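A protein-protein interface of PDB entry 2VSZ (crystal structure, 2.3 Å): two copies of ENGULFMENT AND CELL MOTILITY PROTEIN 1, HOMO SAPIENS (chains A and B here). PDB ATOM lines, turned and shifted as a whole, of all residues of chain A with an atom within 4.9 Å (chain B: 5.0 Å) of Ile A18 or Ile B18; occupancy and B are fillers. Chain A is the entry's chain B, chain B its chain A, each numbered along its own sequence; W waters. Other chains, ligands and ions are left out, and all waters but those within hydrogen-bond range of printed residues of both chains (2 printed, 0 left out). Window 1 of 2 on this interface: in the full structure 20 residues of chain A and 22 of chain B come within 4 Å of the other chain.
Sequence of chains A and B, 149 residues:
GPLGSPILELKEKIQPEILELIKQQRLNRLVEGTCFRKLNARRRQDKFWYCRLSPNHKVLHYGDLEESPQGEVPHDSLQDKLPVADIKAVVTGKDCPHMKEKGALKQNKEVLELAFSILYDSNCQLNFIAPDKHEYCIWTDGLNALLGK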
ATOM      1  N   ILE A  14      33.203 -10.783  23.794  1.00  0.00           N
ATOM      2  CA  ILE A  14      31.958 -11.481  23.527  1.00  0.00           C
ATOM      3  C   ILE A  14      31.036 -11.471  24.781  1.00  0.00           C
ATOM      4  O   ILE A  14      29.873 -11.136  24.683  1.00  0.00           O
ATOM      5  CB  ILE A  14      32.216 -12.955  23.034  1.00  0.00           C
ATOM      6  CG1 ILE A  14      33.081 -12.989  21.747  1.00  0.00           C
ATOM      7  CG2 ILE A  14      30.880 -13.722  22.823  1.00  0.00           C
ATOM      8  CD1 ILE A  14      32.547 -12.140  20.557  1.00  0.00           C
ATOM      9  N   GLN A  15      31.595 -11.820  25.947  1.00  0.00           N
ATOM     10  CA  GLN A  15      30.807 -11.832  27.132  1.00  0.00           C
ATOM     11  C   GLN A  15      30.188 -10.459  27.479  1.00  0.00           C
ATOM     12  O   GLN A  15      29.008 -10.395  27.678  1.00  0.00           O
ATOM     13  CB  GLN A  15      31.564 -12.466  28.314  1.00  0.00           C
ATOM     14  CG  GLN A  15      30.856 -12.226  29.640  1.00  0.00           C
ATOM     15  CD  GLN A  15      31.453 -13.022  30.734  1.00  0.00           C
ATOM     16  OE1 GLN A  15      31.734 -12.499  31.825  1.00  0.00           O
ATOM     17  NE2 GLN A  15      31.658 -14.303  30.477  1.00  0.00           N
ATOM     18  N   PRO A  16      30.975  -9.364  27.555  1.00  0.00           N
ATOM     19  CA  PRO A  16      30.276  -8.095  27.824  1.00  0.00           C
ATOM     20  C   PRO A  16      29.340  -7.596  26.746  1.00  0.00           C
ATOM     21  O   PRO A  16      28.400  -6.839  27.057  1.00  0.00           O
ATOM     22  CB  PRO A  16      31.408  -7.071  28.053  1.00  0.00           C
ATOM     23  CG  PRO A  16      32.684  -7.769  27.463  1.00  0.00           C
ATOM     24  CD  PRO A  16      32.452  -9.231  27.556  1.00  0.00           C
ATOM     25  N   GLU A  17      29.614  -7.926  25.491  1.00  0.00           N
ATOM     26  CA  GLU A  17      28.740  -7.512  24.428  1.00  0.00           C
ATOM     27  C   GLU A  17      27.424  -8.305  24.472  1.00  0.00           C
ATOM     28  O   GLU A  17      26.405  -7.759  24.106  1.00  0.00           O
ATOM     29  CB  GLU A  17      29.365  -7.693  23.070  1.00  0.00           C
ATOM     30  CG  GLU A  17      30.384  -6.631  22.706  1.00  0.00           C
ATOM     31  CD  GLU A  17      31.247  -7.035  21.508  1.00  0.00           C
ATOM     32  OE1 GLU A  17      31.099  -8.162  20.999  1.00  0.00           O
ATOM     33  OE2 GLU A  17      32.084  -6.217  21.064  1.00  0.00           O
ATOM     34  N   ILE A  18      27.472  -9.580  24.859  1.00  0.00           N
ATOM     35  CA  ILE A  18      26.247 -10.320  25.105  1.00  0.00           C
ATOM     36  C   ILE A  18      25.414  -9.775  26.315  1.00  0.00           C
ATOM     37  O   ILE A  18      24.207  -9.608  26.190  1.00  0.00           O
ATOM     38  CB  ILE A  18      26.467 -11.825  25.185  1.00  0.00           C
ATOM     39  CG1 ILE A  18      27.011 -12.365  23.827  1.00  0.00           C
ATOM     40  CG2 ILE A  18      25.104 -12.542  25.590  1.00  0.00           C
ATOM     41  CD1 ILE A  18      27.342 -13.838  23.924  1.00  0.00           C
ATOM     42  N   LEU A  19      26.057  -9.445  27.432  1.00  0.00           N
ATOM     43  CA  LEU A  19      25.327  -8.859  28.562  1.00  0.00           C
ATOM     44  C   LEU A  19      24.744  -7.502  28.196  1.00  0.00           C
ATOM     45  O   LEU A  19      23.655  -7.165  28.662  1.00  0.00           O
ATOM     46  CB  LEU A  19      26.184  -8.745  29.841  1.00  0.00           C
ATOM     47  CG  LEU A  19      26.732 -10.069  30.345  1.00  0.00           C
ATOM     48  CD1 LEU A  19      28.070  -9.918  31.158  1.00  0.00           C
ATOM     49  CD2 LEU A  19      25.734 -10.723  31.152  1.00  0.00           C
ATOM     50  N   GLU A  20      25.464  -6.721  27.391  1.00  0.00           N
ATOM     51  CA  GLU A  20      24.962  -5.451  26.908  1.00  0.00           C
ATOM     52  C   GLU A  20      23.722  -5.541  25.939  1.00  0.00           C
ATOM     53  O   GLU A  20      22.793  -4.739  25.975  1.00  0.00           O
ATOM     54  CB  GLU A  20      26.110  -4.619  26.327  1.00  0.00           C
ATOM     55  CG  GLU A  20      25.673  -3.208  25.942  1.00  0.00           C
ATOM     56  CD  GLU A  20      25.253  -2.337  27.139  1.00  0.00           C
ATOM     57  OE1 GLU A  20      25.613  -2.658  28.318  1.00  0.00           O
ATOM     58  OE2 GLU A  20      24.603  -1.305  26.881  1.00  0.00           O
ATOM     59  N   LEU A  21      23.739  -6.533  25.068  1.00  0.00           N
ATOM     60  CA  LEU A  21      22.631  -6.847  24.209  1.00  0.00           C
ATOM     61  C   LEU A  21      21.330  -7.180  25.016  1.00  0.00           C
ATOM     62  O   LEU A  21      20.254  -6.743  24.672  1.00  0.00           O
ATOM     63  CB  LEU A  21      23.064  -8.114  23.471  1.00  0.00           C
ATOM     64  CG  LEU A  21      23.060  -8.243  21.973  1.00  0.00           C
ATOM     65  CD1 LEU A  21      23.085  -6.895  21.181  1.00  0.00           C
ATOM     66  CD2 LEU A  21      24.216  -9.186  21.567  1.00  0.00           C
ATOM     67  N   ILE A  22      21.476  -8.023  26.025  1.00  0.00           N
ATOM     68  CA  ILE A  22      20.433  -8.520  26.872  1.00  0.00           C
ATOM     69  C   ILE A  22      19.923  -7.323  27.632  1.00  0.00           C
ATOM     70  O   ILE A  22      18.731  -7.044  27.592  1.00  0.00           O
ATOM     71  CB  ILE A  22      20.924  -9.657  27.824  1.00  0.00           C
ATOM     72  CG1 ILE A  22      21.165 -10.951  27.042  1.00  0.00           C
ATOM     73  CG2 ILE A  22      19.893  -9.957  28.971  1.00  0.00           C
ATOM     74  CD1 ILE A  22      21.717 -12.166  27.941  1.00  0.00           C
ATOM     75  N   ILE B  14      18.691 -17.355  30.179  1.00  0.00           N
ATOM     76  CA  ILE B  14      19.615 -17.256  29.088  1.00  0.00           C
ATOM     77  C   ILE B  14      20.943 -16.607  29.588  1.00  0.00           C
ATOM     78  O   ILE B  14      22.050 -17.131  29.304  1.00  0.00           O
ATOM     79  CB  ILE B  14      19.026 -16.495  27.853  1.00  0.00           C
ATOM     80  CG1 ILE B  14      17.715 -17.144  27.345  1.00  0.00           C
ATOM     81  CG2 ILE B  14      20.090 -16.440  26.730  1.00  0.00           C
ATOM     82  CD1 ILE B  14      17.844 -18.618  26.860  1.00  0.00           C
ATOM     83  N   GLN B  15      20.835 -15.503  30.327  1.00  0.00           N
ATOM     84  CA  GLN B  15      22.040 -14.806  30.745  1.00  0.00           C
ATOM     85  C   GLN B  15      22.997 -15.668  31.627  1.00  0.00           C
ATOM     86  O   GLN B  15      24.128 -15.851  31.267  1.00  0.00           O
ATOM     87  CB  GLN B  15      21.737 -13.440  31.348  1.00  0.00           C
ATOM     88  CG  GLN B  15      23.005 -12.751  31.821  1.00  0.00           C
ATOM     89  CD  GLN B  15      22.765 -11.364  32.260  1.00  0.00           C
ATOM     90  OE1 GLN B  15      22.253 -10.562  31.510  1.00  0.00           O
ATOM     91  NE2 GLN B  15      23.168 -11.050  33.487  1.00  0.00           N
ATOM     92  N   PRO B  16      22.491 -16.282  32.715  1.00  0.00           N
ATOM     93  CA  PRO B  16      23.429 -17.133  33.447  1.00  0.00           C
ATOM     94  C   PRO B  16      23.965 -18.376  32.710  1.00  0.00           C
ATOM     95  O   PRO B  16      25.110 -18.839  33.017  1.00  0.00           O
ATOM     96  CB  PRO B  16      22.636 -17.585  34.696  1.00  0.00           C
ATOM     97  CG  PRO B  16      21.235 -16.950  34.594  1.00  0.00           C
ATOM     98  CD  PRO B  16      21.239 -15.986  33.453  1.00  0.00           C
ATOM     99  N   GLU B  17      23.142 -18.971  31.836  1.00  0.00           N
ATOM    100  CA  GLU B  17      23.588 -20.090  31.053  1.00  0.00           C
ATOM    101  C   GLU B  17      24.731 -19.756  30.066  1.00  0.00           C
ATOM    102  O   GLU B  17      25.615 -20.544  29.869  1.00  0.00           O
ATOM    103  CB  GLU B  17      22.419 -20.746  30.328  1.00  0.00           C
ATOM    104  CG  GLU B  17      21.573 -21.636  31.236  1.00  0.00           C
ATOM    105  CD  GLU B  17      20.187 -21.986  30.639  1.00  0.00           C
ATOM    106  OE1 GLU B  17      19.827 -21.489  29.526  1.00  0.00           O
ATOM    107  OE2 GLU B  17      19.452 -22.773  31.302  1.00  0.00           O
ATOM    108  N   ILE B  18      24.649 -18.622  29.418  1.00  0.00           N
ATOM    109  CA  ILE B  18      25.680 -18.130  28.602  1.00  0.00           C
ATOM    110  C   ILE B  18      26.980 -17.826  29.432  1.00  0.00           C
ATOM    111  O   ILE B  18      28.028 -18.168  28.982  1.00  0.00           O
ATOM    112  CB  ILE B  18      25.218 -16.924  27.774  1.00  0.00           C
ATOM    113  CG1 ILE B  18      24.160 -17.376  26.747  1.00  0.00           C
ATOM    114  CG2 ILE B  18      26.422 -16.280  27.019  1.00  0.00           C
ATOM    115  CD1 ILE B  18      23.672 -16.221  25.878  1.00  0.00           C
ATOM    116  N   LEU B  19      26.876 -17.216  30.618  1.00  0.00           N
ATOM    117  CA  LEU B  19      28.040 -16.938  31.445  1.00  0.00           C
ATOM    118  C   LEU B  19      28.690 -18.260  31.859  1.00  0.00           C
ATOM    119  O   LEU B  19      29.888 -18.378  31.833  1.00  0.00           O
ATOM    120  CB  LEU B  19      27.645 -16.109  32.678  1.00  0.00           C
ATOM    121  CG  LEU B  19      27.290 -14.645  32.392  1.00  0.00           C
ATOM    122  CD1 LEU B  19      26.480 -13.995  33.539  1.00  0.00           C
ATOM    123  CD2 LEU B  19      28.586 -13.878  32.146  1.00  0.00           C
ATOM    124  N   GLU B  20      27.868 -19.248  32.230  1.00  0.00           N
ATOM    125  CA  GLU B  20      28.341 -20.539  32.635  1.00  0.00           C
ATOM    126  C   GLU B  20      29.060 -21.222  31.459  1.00  0.00           C
ATOM    127  O   GLU B  20      30.129 -21.823  31.631  1.00  0.00           O
ATOM    128  CB  GLU B  20      27.207 -21.378  33.295  1.00  0.00           C
ATOM    129  CG  GLU B  20      27.602 -22.777  33.820  1.00  0.00           C
ATOM    130  CD  GLU B  20      28.751 -22.774  34.886  1.00  0.00           C
ATOM    131  OE1 GLU B  20      29.097 -21.706  35.441  1.00  0.00           O
ATOM    132  OE2 GLU B  20      29.268 -23.852  35.206  1.00  0.00           O
ATOM    133  N   LEU B  21      28.534 -21.130  30.248  1.00  0.00           N
ATOM    134  CA  LEU B  21      29.195 -21.861  29.203  1.00  0.00           C
ATOM    135  C   LEU B  21      30.542 -21.257  28.752  1.00  0.00           C
ATOM    136  O   LEU B  21      31.422 -21.971  28.239  1.00  0.00           O
ATOM    137  CB  LEU B  21      28.234 -22.146  28.074  1.00  0.00           C
ATOM    138  CG  LEU B  21      28.016 -21.600  26.675  1.00  0.00           C
ATOM    139  CD1 LEU B  21      26.460 -21.630  26.504  1.00  0.00           C
ATOM    140  CD2 LEU B  21      28.512 -20.207  26.491  1.00  0.00           C
ATOM    141  N   ILE B  22      30.661 -19.946  28.912  1.00  0.00           N
ATOM    142  CA  ILE B  22      31.852 -19.223  28.662  1.00  0.00           C
ATOM    143  C   ILE B  22      32.887 -19.532  29.788  1.00  0.00           C
ATOM    144  O   ILE B  22      34.022 -19.810  29.470  1.00  0.00           O
ATOM    145  CB  ILE B  22      31.565 -17.724  28.544  1.00  0.00           C
ATOM    146  CG1 ILE B  22      30.842 -17.408  27.212  1.00  0.00           C
ATOM    147  CG2 ILE B  22      32.893 -16.901  28.639  1.00  0.00           C
ATOM    148  CD1 ILE B  22      30.483 -15.905  27.024  1.00  0.00           C
HETATM  149  O   HOH W   1      31.224 -16.462  33.061  1.00  0.00           O
HETATM  150  O   HOH W   2      22.664  -7.990  31.152  1.00  0.00           O
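Among the printed residues, pairs that only touch across the chains: Leu A19 with Gln B15 (3.2 Å), Gln A15 with Leu B19 (3.3 Å), Gln A15 with Ile B22 (3.4 Å), Ile A22 with Gln B15 (3.5 Å) and Ile A18 with Ile B18 (3.96 Å).
Ile B18 touches just one residue of chain A: Ile A18 (3.96 Å). Of the printed residues of chain A, Ile B22 touches Gln A15 (3.4 Å). Of the printed residues of chain B, Ile A22 touches Gln B15. Of the printed residues of chain A, Gln B15 touches Leu A19 and Ile A22. Printed residues of chain A within 4 Å of Leu B19: Gln A15. Ile A14 touches none of the printed residues of chain B. The nearest printed residue of chain A that does not touch Ile B18 is Ile A22 (5.0 Å).
Among the printed residues, 5 pairs touch across the chains.
Gln A15 touches Leu B19, and with the chains exchanged Leu A19 touches Gln B15. Gln A15 touches Ile B22, and with the chains exchanged Ile A22 touches Gln B15. Ile A18 touches its own counterpart, Ile B18. Positions printed for both chains: 14, 15, 16, 17, 18, 19, 20, 21 and 22. Of the 5 pairs that touch across the chains among the printed residues, 5 have their exchanged pair printed and touching as well.
Water W2 lies within hydrogen-bond range of the side-chain amide oxygen of Gln B15 (2.6 Å) and the backbone carbonyl oxygen of Leu A19 (2.8 Å). Water W1 lies within hydrogen-bond range of O of Leu B19 (2.6 Å) and NE2 of Gln A15 (3.4 Å).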
